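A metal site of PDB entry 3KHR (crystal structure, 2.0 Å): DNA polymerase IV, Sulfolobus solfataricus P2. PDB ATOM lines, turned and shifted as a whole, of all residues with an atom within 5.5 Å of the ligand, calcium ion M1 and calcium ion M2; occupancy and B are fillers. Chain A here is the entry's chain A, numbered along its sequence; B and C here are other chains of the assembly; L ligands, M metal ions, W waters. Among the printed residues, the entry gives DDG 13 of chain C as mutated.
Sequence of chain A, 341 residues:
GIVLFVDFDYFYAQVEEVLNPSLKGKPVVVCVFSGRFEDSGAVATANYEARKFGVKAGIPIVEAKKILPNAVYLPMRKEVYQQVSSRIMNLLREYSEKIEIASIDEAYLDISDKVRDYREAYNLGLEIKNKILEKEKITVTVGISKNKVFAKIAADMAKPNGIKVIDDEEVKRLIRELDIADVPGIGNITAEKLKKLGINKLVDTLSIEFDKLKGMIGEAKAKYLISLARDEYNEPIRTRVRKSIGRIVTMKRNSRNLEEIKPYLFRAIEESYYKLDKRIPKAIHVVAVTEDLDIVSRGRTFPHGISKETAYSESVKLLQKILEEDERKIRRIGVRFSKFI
OG1 of Thr 45 sits at hydrogen-bond distance from O5 of the ligand (2.7 Å). N of Tyr 12 sits at hydrogen-bond distance from O12 of the ligand. A nitrogen (N2) of the ligand is in hydrogen-bond range of N1 of DA 4 of chain B, at 2.7 Å. O7 of the ligand lies within hydrogen-bond range of OH of Tyr 48 (2.8 Å). NZ of Lys 159 is in salt-bridge range of O8 of the ligand (3.6 Å). A nitrogen (N2) of the ligand lies close to the backbone carbonyl oxygen (O) of Ala 44, 3.4 Å away. N of Tyr 10 lies within hydrogen-bond range of O7 of the ligand (2.9 Å). An oxygen (O5) of the ligand is in hydrogen-bond range of the backbone NH (N) of Phe 11. An oxygen (O8) of the ligand lies within salt-bridge range of the guanidinium group (NH1) of Arg 51 (2.9 Å).
The side-chain amino group (NZ) of Lys 152 lies within salt-bridge range of the side-chain carboxylate (OE2) of Glu 106 (2.8 Å). OP1 of DDG 13 of chain C lies within salt-bridge range of the side-chain amino group (NZ) of Lys 152 (3.1 Å). The side-chain hydroxyl of Ser 103 sits close to the backbone NH of Asp 105, at 3.3 Å. The side-chain hydroxyl (OG) of Ser 103 lies within hydrogen-bond range of the side-chain carboxylate (OE1) of Glu 106 (3.2 Å). OD2 of Asp 7 is in salt-bridge range of NZ of Lys 159, 2.9 Å away. The side-chain hydroxyl (OG1) of Thr 45 is in hydrogen-bond range of the guanidinium group (NH2) of Arg 51 (3.2 Å). N2 of DDG 13 of chain C lies close to O2 of DC 5 of chain B, 2.7 Å away. NE of Arg 51 sits at hydrogen-bond distance from O of Ala 46, 2.8 Å away.
O14 of the ligand lies close to O6 of DDG 13 of chain C, at 3.3 Å. Residues that only touch the ligand: Ala 57 (3.5 Å) and Asp 9 (3.8 Å). Hydrophobic or aromatic side chains that line the ligand: Phe 11, Tyr 12, Ala 44, Tyr 48 and Ala 57. 15 residues have an atom within 4 Å of the ligand: Asp 7, Phe 8, Asp 9, Tyr 10, Phe 11, Tyr 12, Ala 44, Thr 45, Tyr 48, Arg 51, Ala 57, Asp 105, Lys 159, DA 4 of chain B and DDG 13 of chain C.
Within 4 Å of calcium ion M1: Asp 7, Phe 8 and Asp 105. The nearest printed residue that does not touch calcium ion M1 is Lys 159 (4.02 Å).
Residues that only touch calcium ion M2: Glu 106 (3.2 Å) and DDG 13 of chain C (3.5 Å). Along chain A the residues within 4 Å of calcium ion M2 span positions 7 to 106.
Calcium ion M1 is bound by the side-chain carboxylate (OD1) of Asp 7 (2.3 Å), the backbone carbonyl oxygen (O) of Phe 8 (2.3 Å), an oxygen (O4) of the ligand (2.3 Å), the side-chain carboxylate (OD2) of Asp 105 (2.3 Å), an oxygen (O1) of the ligand (2.3 Å) and an oxygen (O9) of the ligand (2.4 Å). Calcium ion M1 has six donor atoms within binding distance.
Calcium ion M2 is bound by water W1, O1 of the ligand and OD1 of Asp 105. Calcium ion M2 has three donor atoms within binding distance.
Water W1 bridges OD2 of Asp 7 (2.5 Å) and NZ of Lys 152 (3.3 Å). Water W3 lies within hydrogen-bond range of an oxygen (O13) of the ligand (2.7 Å), the side-chain hydroxyl of Tyr 12 (2.8 Å) and N2 of DDG 13 of chain C (3.5 Å). Water W4 bridges O3 of the ligand (2.9 Å) and OG1 of Thr 45 (3.5 Å). Water W2 lies within hydrogen-bond range of the side-chain carboxylate of Asp 9 (3.1 Å), the backbone carbonyl oxygen of Asp 7 (3.3 Å) and an oxygen (O7) of the ligand (3.3 Å).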
ATOM      1  N   ASP A   7     -27.058  32.059 -14.065  1.00  0.00           N
ATOM      2  CA  ASP A   7     -25.860  31.475 -13.471  1.00  0.00           C
ATOM      3  C   ASP A   7     -24.964  32.691 -13.080  1.00  0.00           C
ATOM      4  O   ASP A   7     -24.548  33.489 -13.955  1.00  0.00           O
ATOM      5  CB  ASP A   7     -25.223  30.542 -14.517  1.00  0.00           C
ATOM      6  CG  ASP A   7     -23.938  29.862 -14.040  1.00  0.00           C
ATOM      7  OD1 ASP A   7     -23.215  30.486 -13.261  1.00  0.00           O
ATOM      8  OD2 ASP A   7     -23.617  28.720 -14.502  1.00  0.00           O
ATOM      9  N   PHE A   8     -24.690  32.856 -11.777  1.00  0.00           N
ATOM     10  CA  PHE A   8     -24.035  34.078 -11.278  1.00  0.00           C
ATOM     11  C   PHE A   8     -22.550  34.008 -11.601  1.00  0.00           C
ATOM     12  O   PHE A   8     -21.973  32.939 -11.480  1.00  0.00           O
ATOM     13  CB  PHE A   8     -24.205  34.291  -9.749  1.00  0.00           C
ATOM     14  CG  PHE A   8     -25.623  34.124  -9.242  1.00  0.00           C
ATOM     15  CD1 PHE A   8     -26.723  34.214 -10.081  1.00  0.00           C
ATOM     16  CD2 PHE A   8     -25.843  33.914  -7.885  1.00  0.00           C
ATOM     17  CE1 PHE A   8     -28.040  34.038  -9.595  1.00  0.00           C
ATOM     18  CE2 PHE A   8     -27.145  33.731  -7.381  1.00  0.00           C
ATOM     19  CZ  PHE A   8     -28.237  33.802  -8.247  1.00  0.00           C
ATOM     20  N   ASP A   9     -21.938  35.127 -12.019  1.00  0.00           N
ATOM     21  CA  ASP A   9     -20.548  35.096 -12.523  1.00  0.00           C
ATOM     22  C   ASP A   9     -19.523  35.010 -11.380  1.00  0.00           C
ATOM     23  O   ASP A   9     -19.597  35.758 -10.403  1.00  0.00           O
ATOM     24  CB  ASP A   9     -20.205  36.321 -13.410  1.00  0.00           C
ATOM     25  CG  ASP A   9     -21.107  36.465 -14.646  1.00  0.00           C
ATOM     26  OD1 ASP A   9     -21.483  35.462 -15.299  1.00  0.00           O
ATOM     27  OD2 ASP A   9     -21.458  37.622 -14.978  1.00  0.00           O
ATOM     28  N   TYR A  10     -18.545  34.117 -11.520  1.00  0.00           N
ATOM     29  CA  TYR A  10     -17.486  33.858 -10.531  1.00  0.00           C
ATOM     30  C   TYR A  10     -17.942  34.122  -9.097  1.00  0.00           C
ATOM     31  O   TYR A  10     -17.329  34.901  -8.353  1.00  0.00           O
ATOM     32  CB  TYR A  10     -16.171  34.592 -10.892  1.00  0.00           C
ATOM     33  CG  TYR A  10     -16.255  36.130 -11.002  1.00  0.00           C
ATOM     34  CD1 TYR A  10     -15.651  36.953 -10.025  1.00  0.00           C
ATOM     35  CD2 TYR A  10     -16.885  36.733 -12.081  1.00  0.00           C
ATOM     36  CE1 TYR A  10     -15.708  38.338 -10.136  1.00  0.00           C
ATOM     37  CE2 TYR A  10     -16.957  38.108 -12.193  1.00  0.00           C
ATOM     38  CZ  TYR A  10     -16.368  38.899 -11.223  1.00  0.00           C
ATOM     39  OH  TYR A  10     -16.470  40.250 -11.359  1.00  0.00           O
ATOM     40  N   PHE A  11     -19.048  33.460  -8.712  1.00  0.00           N
ATOM     41  CA  PHE A  11     -19.898  33.985  -7.633  1.00  0.00           C
ATOM     42  C   PHE A  11     -19.197  34.407  -6.335  1.00  0.00           C
ATOM     43  O   PHE A  11     -19.325  35.566  -5.960  1.00  0.00           O
ATOM     44  CB  PHE A  11     -21.126  33.068  -7.376  1.00  0.00           C
ATOM     45  CG  PHE A  11     -22.117  33.637  -6.399  1.00  0.00           C
ATOM     46  CD1 PHE A  11     -22.528  34.972  -6.486  1.00  0.00           C
ATOM     47  CD2 PHE A  11     -22.640  32.828  -5.396  1.00  0.00           C
ATOM     48  CE1 PHE A  11     -23.440  35.495  -5.573  1.00  0.00           C
ATOM     49  CE2 PHE A  11     -23.554  33.336  -4.453  1.00  0.00           C
ATOM     50  CZ  PHE A  11     -23.966  34.664  -4.547  1.00  0.00           C
ATOM     51  N   TYR A  12     -18.496  33.505  -5.641  1.00  0.00           N
ATOM     52  CA  TYR A  12     -17.916  33.844  -4.326  1.00  0.00           C
ATOM     53  C   TYR A  12     -16.910  34.993  -4.416  1.00  0.00           C
ATOM     54  O   TYR A  12     -16.937  35.922  -3.588  1.00  0.00           O
ATOM     55  CB  TYR A  12     -17.233  32.629  -3.678  1.00  0.00           C
ATOM     56  CG  TYR A  12     -18.146  31.498  -3.246  1.00  0.00           C
ATOM     57  CD1 TYR A  12     -19.502  31.522  -3.517  1.00  0.00           C
ATOM     58  CD2 TYR A  12     -17.608  30.384  -2.583  1.00  0.00           C
ATOM     59  CE1 TYR A  12     -20.323  30.449  -3.126  1.00  0.00           C
ATOM     60  CE2 TYR A  12     -18.402  29.313  -2.217  1.00  0.00           C
ATOM     61  CZ  TYR A  12     -19.760  29.362  -2.468  1.00  0.00           C
ATOM     62  OH  TYR A  12     -20.543  28.302  -2.072  1.00  0.00           O
ATOM     63  N   ALA A  13     -16.014  34.925  -5.398  1.00  0.00           N
ATOM     64  CA  ALA A  13     -15.028  35.981  -5.621  1.00  0.00           C
ATOM     65  C   ALA A  13     -15.692  37.328  -5.960  1.00  0.00           C
ATOM     66  O   ALA A  13     -15.273  38.389  -5.449  1.00  0.00           O
ATOM     67  CB  ALA A  13     -14.042  35.556  -6.752  1.00  0.00           C
ATOM     68  N   VAL A  43      -9.103  25.422  -3.468  1.00  0.00           N
ATOM     69  CA  VAL A  43      -9.748  26.627  -3.974  1.00  0.00           C
ATOM     70  C   VAL A  43     -11.219  26.369  -4.235  1.00  0.00           C
ATOM     71  O   VAL A  43     -11.566  25.383  -4.884  1.00  0.00           O
ATOM     72  CB  VAL A  43      -9.056  27.081  -5.308  1.00  0.00           C
ATOM     73  CG1 VAL A  43      -9.858  28.172  -6.001  1.00  0.00           C
ATOM     74  CG2 VAL A  43      -7.612  27.540  -5.051  1.00  0.00           C
ATOM     75  N   ALA A  44     -12.097  27.260  -3.779  1.00  0.00           N
ATOM     76  CA  ALA A  44     -13.530  27.157  -4.088  1.00  0.00           C
ATOM     77  C   ALA A  44     -13.833  27.775  -5.450  1.00  0.00           C
ATOM     78  O   ALA A  44     -14.639  27.213  -6.223  1.00  0.00           O
ATOM     79  CB  ALA A  44     -14.400  27.816  -2.978  1.00  0.00           C
ATOM     80  N   THR A  45     -13.256  28.949  -5.711  1.00  0.00           N
ATOM     81  CA  THR A  45     -13.342  29.588  -7.028  1.00  0.00           C
ATOM     82  C   THR A  45     -12.336  30.729  -7.139  1.00  0.00           C
ATOM     83  O   THR A  45     -11.655  31.036  -6.166  1.00  0.00           O
ATOM     84  CB  THR A  45     -14.763  30.154  -7.367  1.00  0.00           C
ATOM     85  OG1 THR A  45     -14.796  30.508  -8.750  1.00  0.00           O
ATOM     86  CG2 THR A  45     -15.070  31.406  -6.559  1.00  0.00           C
ATOM     87  N   ALA A  46     -12.257  31.344  -8.323  1.00  0.00           N
ATOM     88  CA  ALA A  46     -11.392  32.505  -8.470  1.00  0.00           C
ATOM     89  C   ALA A  46     -11.972  33.374  -9.552  1.00  0.00           C
ATOM     90  O   ALA A  46     -12.696  32.875 -10.425  1.00  0.00           O
ATOM     91  CB  ALA A  46      -9.965  32.087  -8.835  1.00  0.00           C
ATOM     92  N   TYR A  48     -11.898  35.892 -12.944  1.00  0.00           N
ATOM     93  CA  TYR A  48     -11.363  35.582 -14.256  1.00  0.00           C
ATOM     94  C   TYR A  48      -9.910  35.998 -14.417  1.00  0.00           C
ATOM     95  O   TYR A  48      -9.156  35.354 -15.151  1.00  0.00           O
ATOM     96  CB  TYR A  48     -12.283  36.135 -15.359  1.00  0.00           C
ATOM     97  CG  TYR A  48     -13.462  35.211 -15.582  1.00  0.00           C
ATOM     98  CD1 TYR A  48     -14.545  35.204 -14.700  1.00  0.00           C
ATOM     99  CD2 TYR A  48     -13.475  34.316 -16.661  1.00  0.00           C
ATOM    100  CE1 TYR A  48     -15.636  34.340 -14.879  1.00  0.00           C
ATOM    101  CE2 TYR A  48     -14.579  33.443 -16.855  1.00  0.00           C
ATOM    102  CZ  TYR A  48     -15.651  33.462 -15.960  1.00  0.00           C
ATOM    103  OH  TYR A  48     -16.736  32.611 -16.138  1.00  0.00           O
ATOM    104  N   ARG A  51      -7.931  33.140 -13.180  1.00  0.00           N
ATOM    105  CA  ARG A  51      -8.076  31.940 -14.022  1.00  0.00           C
ATOM    106  C   ARG A  51      -7.158  31.955 -15.221  1.00  0.00           C
ATOM    107  O   ARG A  51      -6.814  30.889 -15.735  1.00  0.00           O
ATOM    108  CB  ARG A  51      -9.517  31.738 -14.490  1.00  0.00           C
ATOM    109  CG  ARG A  51     -10.492  31.444 -13.344  1.00  0.00           C
ATOM    110  CD  ARG A  51     -11.907  31.246 -13.880  1.00  0.00           C
ATOM    111  NE  ARG A  51     -12.883  31.462 -12.805  1.00  0.00           N
ATOM    112  CZ  ARG A  51     -14.177  31.213 -12.898  1.00  0.00           C
ATOM    113  NH1 ARG A  51     -14.692  30.685 -14.018  1.00  0.00           N
ATOM    114  NH2 ARG A  51     -14.958  31.453 -11.846  1.00  0.00           N
ATOM    115  N   ALA A  57     -11.409  26.294  -9.414  1.00  0.00           N
ATOM    116  CA  ALA A  57     -12.048  25.517  -8.365  1.00  0.00           C
ATOM    117  C   ALA A  57     -11.393  24.143  -8.183  1.00  0.00           C
ATOM    118  O   ALA A  57     -11.096  23.461  -9.160  1.00  0.00           O
ATOM    119  CB  ALA A  57     -13.565  25.383  -8.663  1.00  0.00           C
ATOM    120  N   GLY A  58     -11.088  23.760  -6.952  1.00  0.00           N
ATOM    121  CA  GLY A  58     -10.620  22.413  -6.655  1.00  0.00           C
ATOM    122  C   GLY A  58      -9.124  22.165  -6.578  1.00  0.00           C
ATOM    123  O   GLY A  58      -8.696  21.167  -5.996  1.00  0.00           O
ATOM    124  N   MET A  76     -13.048  31.309   2.372  1.00  0.00           N
ATOM    125  CA  MET A  76     -14.442  31.210   1.918  1.00  0.00           C
ATOM    126  C   MET A  76     -15.391  31.516   3.084  1.00  0.00           C
ATOM    127  O   MET A  76     -15.307  30.862   4.129  1.00  0.00           O
ATOM    128  CB  MET A  76     -14.717  29.814   1.336  1.00  0.00           C
ATOM    129  CG  MET A  76     -16.138  29.618   0.842  1.00  0.00           C
ATOM    130  SD  MET A  76     -16.611  27.901   0.633  1.00  0.00           S
ATOM    131  CE  MET A  76     -16.480  27.223   2.289  1.00  0.00           C
ATOM    132  N   SER A 103     -28.773  25.421  -7.342  1.00  0.00           N
ATOM    133  CA  SER A 103     -27.609  25.488  -6.446  1.00  0.00           C
ATOM    134  C   SER A 103     -27.519  26.880  -5.848  1.00  0.00           C
ATOM    135  O   SER A 103     -28.402  27.712  -6.091  1.00  0.00           O
ATOM    136  CB  SER A 103     -26.319  25.223  -7.207  1.00  0.00           C
ATOM    137  OG  SER A 103     -26.118  26.281  -8.131  1.00  0.00           O
ATOM    138  N   ILE A 104     -26.438  27.176  -5.124  1.00  0.00           N
ATOM    139  CA  ILE A 104     -26.242  28.501  -4.549  1.00  0.00           C
ATOM    140  C   ILE A 104     -26.263  29.626  -5.617  1.00  0.00           C
ATOM    141  O   ILE A 104     -26.572  30.762  -5.296  1.00  0.00           O
ATOM    142  CB  ILE A 104     -24.947  28.599  -3.665  1.00  0.00           C
ATOM    143  CG1 ILE A 104     -25.043  29.789  -2.701  1.00  0.00           C
ATOM    144  CG2 ILE A 104     -23.679  28.666  -4.545  1.00  0.00           C
ATOM    145  CD1 ILE A 104     -24.208  29.677  -1.447  1.00  0.00           C
ATOM    146  N   ASP A 105     -25.970  29.306  -6.863  1.00  0.00           N
ATOM    147  CA  ASP A 105     -25.886  30.389  -7.878  1.00  0.00           C
ATOM    148  C   ASP A 105     -26.524  30.117  -9.256  1.00  0.00           C
ATOM    149  O   ASP A 105     -26.177  30.775 -10.246  1.00  0.00           O
ATOM    150  CB  ASP A 105     -24.415  30.875  -8.012  1.00  0.00           C
ATOM    151  CG  ASP A 105     -23.620  30.087  -9.046  1.00  0.00           C
ATOM    152  OD1 ASP A 105     -23.905  28.891  -9.220  1.00  0.00           O
ATOM    153  OD2 ASP A 105     -22.736  30.675  -9.709  1.00  0.00           O
ATOM    154  N   GLU A 106     -27.475  29.178  -9.287  1.00  0.00           N
ATOM    155  CA  GLU A 106     -28.185  28.767 -10.508  1.00  0.00           C
ATOM    156  C   GLU A 106     -29.663  28.661 -10.258  1.00  0.00           C
ATOM    157  O   GLU A 106     -30.068  28.046  -9.265  1.00  0.00           O
ATOM    158  CB  GLU A 106     -27.776  27.355 -10.932  1.00  0.00           C
ATOM    159  CG  GLU A 106     -26.360  27.131 -11.283  1.00  0.00           C
ATOM    160  CD  GLU A 106     -26.102  25.690 -11.634  1.00  0.00           C
ATOM    161  OE1 GLU A 106     -26.551  24.775 -10.892  1.00  0.00           O
ATOM    162  OE2 GLU A 106     -25.427  25.453 -12.658  1.00  0.00           O
ATOM    163  N   LYS A 152     -28.718  25.718 -20.067  1.00  0.00           N
ATOM    164  CA  LYS A 152     -27.488  25.714 -19.293  1.00  0.00           C
ATOM    165  C   LYS A 152     -26.281  25.818 -20.234  1.00  0.00           C
ATOM    166  O   LYS A 152     -25.333  26.579 -19.970  1.00  0.00           O
ATOM    167  CB  LYS A 152     -27.386  24.448 -18.425  1.00  0.00           C
ATOM    168  CG  LYS A 152     -26.172  24.445 -17.489  1.00  0.00           C
ATOM    169  CD  LYS A 152     -26.154  23.179 -16.654  1.00  0.00           C
ATOM    170  CE  LYS A 152     -25.974  23.468 -15.187  1.00  0.00           C
ATOM    171  NZ  LYS A 152     -24.618  23.930 -14.864  1.00  0.00           N
ATOM    172  N   LYS A 159     -20.710  32.965 -20.873  1.00  0.00           N
ATOM    173  CA  LYS A 159     -20.002  33.313 -19.620  1.00  0.00           C
ATOM    174  C   LYS A 159     -18.725  34.112 -19.904  1.00  0.00           C
ATOM    175  O   LYS A 159     -18.050  33.797 -20.880  1.00  0.00           O
ATOM    176  CB  LYS A 159     -19.608  32.033 -18.851  1.00  0.00           C
ATOM    177  CG  LYS A 159     -20.628  31.510 -17.882  1.00  0.00           C
ATOM    178  CD  LYS A 159     -20.034  30.423 -16.962  1.00  0.00           C
ATOM    179  CE  LYS A 159     -21.157  29.596 -16.295  1.00  0.00           C
ATOM    180  NZ  LYS A 159     -20.733  28.740 -15.122  1.00  0.00           N
ATOM    181  N   PRO A 160     -18.386  35.141 -19.094  1.00  0.00           N
ATOM    182  CA  PRO A 160     -19.151  35.781 -17.996  1.00  0.00           C
ATOM    183  C   PRO A 160     -19.969  36.983 -18.491  1.00  0.00           C
ATOM    184  O   PRO A 160     -19.742  37.463 -19.601  1.00  0.00           O
ATOM    185  CB  PRO A 160     -18.042  36.267 -17.051  1.00  0.00           C
ATOM    186  CG  PRO A 160     -16.889  36.633 -17.990  1.00  0.00           C
ATOM    187  CD  PRO A 160     -17.020  35.701 -19.199  1.00  0.00           C
ATOM    188  P    DA B   4      -9.053  17.847   0.224  1.00  0.00           P
ATOM    189  OP1  DA B   4      -8.269  17.524   1.442  1.00  0.00           O
ATOM    190  OP2  DA B   4      -9.945  16.856  -0.403  1.00  0.00           O
ATOM    191  O5'  DA B   4      -9.885  19.180   0.477  1.00  0.00           O
ATOM    192  C5'  DA B   4      -9.282  20.286   1.148  1.00  0.00           C
ATOM    193  C4'  DA B   4     -10.377  21.116   1.770  1.00  0.00           C
ATOM    194  O4'  DA B   4     -11.109  21.862   0.767  1.00  0.00           O
ATOM    195  C3'  DA B   4     -11.445  20.303   2.480  1.00  0.00           C
ATOM    196  O3'  DA B   4     -11.846  21.051   3.594  1.00  0.00           O
ATOM    197  C2'  DA B   4     -12.576  20.118   1.461  1.00  0.00           C
ATOM    198  C1'  DA B   4     -12.425  21.372   0.588  1.00  0.00           C
ATOM    199  N9   DA B   4     -12.575  21.179  -0.853  1.00  0.00           N
ATOM    200  C8   DA B   4     -11.935  20.293  -1.659  1.00  0.00           C
ATOM    201  N7   DA B   4     -12.281  20.390  -2.927  1.00  0.00           N
ATOM    202  C5   DA B   4     -13.211  21.417  -2.946  1.00  0.00           C
ATOM    203  C6   DA B   4     -13.961  22.038  -3.993  1.00  0.00           C
ATOM    204  N6   DA B   4     -13.902  21.658  -5.284  1.00  0.00           N
ATOM    205  N1   DA B   4     -14.802  23.052  -3.670  1.00  0.00           N
ATOM    206  C2   DA B   4     -14.887  23.421  -2.389  1.00  0.00           C
ATOM    207  N3   DA B   4     -14.208  22.929  -1.347  1.00  0.00           N
ATOM    208  C4   DA B   4     -13.397  21.920  -1.683  1.00  0.00           C
ATOM    209  P    DC B   5     -12.680  20.336   4.768  1.00  0.00           P
ATOM    210  OP1  DC B   5     -12.547  21.196   5.961  1.00  0.00           O
ATOM    211  OP2  DC B   5     -12.256  18.924   4.827  1.00  0.00           O
ATOM    212  O5'  DC B   5     -14.167  20.376   4.205  1.00  0.00           O
ATOM    213  C5'  DC B   5     -14.826  21.642   4.001  1.00  0.00           C
ATOM    214  C4'  DC B   5     -16.093  21.459   3.177  1.00  0.00           C
ATOM    215  O4'  DC B   5     -15.767  21.399   1.754  1.00  0.00           O
ATOM    216  C3'  DC B   5     -16.897  20.182   3.492  1.00  0.00           C
ATOM    217  O3'  DC B   5     -18.314  20.400   3.450  1.00  0.00           O
ATOM    218  C2'  DC B   5     -16.580  19.294   2.281  1.00  0.00           C
ATOM    219  C1'  DC B   5     -16.611  20.401   1.219  1.00  0.00           C
ATOM    220  N1   DC B   5     -16.271  19.949  -0.140  1.00  0.00           N
ATOM    221  C2   DC B   5     -16.895  20.611  -1.221  1.00  0.00           C
ATOM    222  O2   DC B   5     -17.696  21.529  -1.000  1.00  0.00           O
ATOM    223  N3   DC B   5     -16.626  20.185  -2.485  1.00  0.00           N
ATOM    224  C4   DC B   5     -15.768  19.185  -2.686  1.00  0.00           C
ATOM    225  N4   DC B   5     -15.538  18.818  -3.952  1.00  0.00           N
ATOM    226  C5   DC B   5     -15.108  18.506  -1.598  1.00  0.00           C
ATOM    227  C6   DC B   5     -15.420  18.905  -0.353  1.00  0.00           C
ATOM    228  P   DDG C  13     -22.709  22.508 -12.325  1.00  0.00           P
ATOM    229  OP1 DDG C  13     -24.026  21.870 -12.588  1.00  0.00           O
ATOM    230  OP2 DDG C  13     -21.921  23.119 -13.398  1.00  0.00           O
ATOM    231  O5' DDG C  13     -22.821  23.650 -11.210  1.00  0.00           O
ATOM    232  C5' DDG C  13     -23.771  23.611 -10.206  1.00  0.00           C
ATOM    233  C4' DDG C  13     -23.220  24.145  -8.902  1.00  0.00           C
ATOM    234  O4' DDG C  13     -22.628  23.044  -8.196  1.00  0.00           O
ATOM    235  C3' DDG C  13     -22.042  25.117  -8.984  1.00  0.00           C
ATOM    236  C2' DDG C  13     -21.521  25.069  -7.558  1.00  0.00           C
ATOM    237  C1' DDG C  13     -21.712  23.591  -7.255  1.00  0.00           C
ATOM    238  N9  DDG C  13     -20.551  22.728  -7.335  1.00  0.00           N
ATOM    239  C8  DDG C  13     -20.003  22.066  -8.406  1.00  0.00           C
ATOM    240  N7  DDG C  13     -18.965  21.332  -8.076  1.00  0.00           N
ATOM    241  C5  DDG C  13     -18.832  21.533  -6.709  1.00  0.00           C
ATOM    242  C6  DDG C  13     -17.913  21.004  -5.787  1.00  0.00           C
ATOM    243  O6  DDG C  13     -16.977  20.225  -6.013  1.00  0.00           O
ATOM    244  N1  DDG C  13     -18.140  21.480  -4.499  1.00  0.00           N
ATOM    245  C2  DDG C  13     -19.156  22.351  -4.141  1.00  0.00           C
ATOM    246  N2  DDG C  13     -19.259  22.729  -2.864  1.00  0.00           N
ATOM    247  N3  DDG C  13     -20.026  22.841  -4.996  1.00  0.00           N
ATOM    248  C4  DDG C  13     -19.796  22.387  -6.249  1.00  0.00           C
HETATM  249  P1  LIG L   1     -19.765  27.916 -10.549  1.00  0.00           P
HETATM  250  O1  LIG L   1     -21.022  28.489 -11.158  1.00  0.00           O
HETATM  251  O2  LIG L   1     -19.290  26.614 -11.114  1.00  0.00           O
HETATM  252  O3  LIG L   1     -18.457  28.849 -10.644  1.00  0.00           O
HETATM  253  P2  LIG L   1     -18.394  30.450 -10.530  1.00  0.00           P
HETATM  254  O4  LIG L   1     -19.715  31.155 -10.362  1.00  0.00           O
HETATM  255  O5  LIG L   1     -17.362  30.808  -9.495  1.00  0.00           O
HETATM  256  O6  LIG L   1     -17.686  30.794 -11.933  1.00  0.00           O
HETATM  257  P3  LIG L   1     -18.391  30.947 -13.364  1.00  0.00           P
HETATM  258  O7  LIG L   1     -18.327  32.376 -13.840  1.00  0.00           O
HETATM  259  O8  LIG L   1     -17.518  30.207 -14.325  1.00  0.00           O
HETATM  260  O9  LIG L   1     -19.825  30.482 -13.376  1.00  0.00           O
HETATM  261  O10 LIG L   1     -19.892  27.701  -8.970  1.00  0.00           O
HETATM  262  C1  LIG L   1     -20.617  28.644  -8.166  1.00  0.00           C
HETATM  263  C2  LIG L   1     -19.941  28.749  -6.821  1.00  0.00           C
HETATM  264  O11 LIG L   1     -19.914  27.487  -6.151  1.00  0.00           O
HETATM  265  C3  LIG L   1     -18.493  29.214  -6.943  1.00  0.00           C
HETATM  266  O12 LIG L   1     -18.385  30.645  -7.033  1.00  0.00           O
HETATM  267  C4  LIG L   1     -17.870  28.647  -5.668  1.00  0.00           C
HETATM  268  C5  LIG L   1     -18.697  27.373  -5.407  1.00  0.00           C
HETATM  269  N1  LIG L   1     -17.911  26.212  -5.886  1.00  0.00           N
HETATM  270  C6  LIG L   1     -17.159  25.457  -4.951  1.00  0.00           C
HETATM  271  O13 LIG L   1     -17.152  25.782  -3.741  1.00  0.00           O
HETATM  272  N2  LIG L   1     -16.431  24.410  -5.368  1.00  0.00           N
HETATM  273  C7  LIG L   1     -16.374  24.047  -6.660  1.00  0.00           C
HETATM  274  O14 LIG L   1     -15.687  23.074  -7.023  1.00  0.00           O
HETATM  275  C8  LIG L   1     -17.164  24.812  -7.665  1.00  0.00           C
HETATM  276  C9  LIG L   1     -17.172  24.465  -9.125  1.00  0.00           C
HETATM  277  C10 LIG L   1     -17.911  25.892  -7.189  1.00  0.00           C
HETATM  278 CA    CA M   1     -21.540  30.692 -11.707  1.00  0.00          CA
HETATM  279 CA    CA M   2     -23.158  27.507 -11.215  1.00  0.00          CA
HETATM  280  O   HOH W   1     -23.472  26.523 -13.235  1.00  0.00           O
HETATM  281  O   HOH W   2     -21.526  32.446 -14.804  1.00  0.00           O
HETATM  282  O   HOH W   3     -18.978  26.005  -1.723  1.00  0.00           O
HETATM  283  O   HOH W   4     -15.798  27.713 -10.595  1.00  0.00           O
HETATM  284  O   HOH W   5     -14.737  21.758  -9.086  1.00  0.00           O
HETATM  285  O   HOH W   6     -17.113  27.817 -14.532  1.00  0.00           O
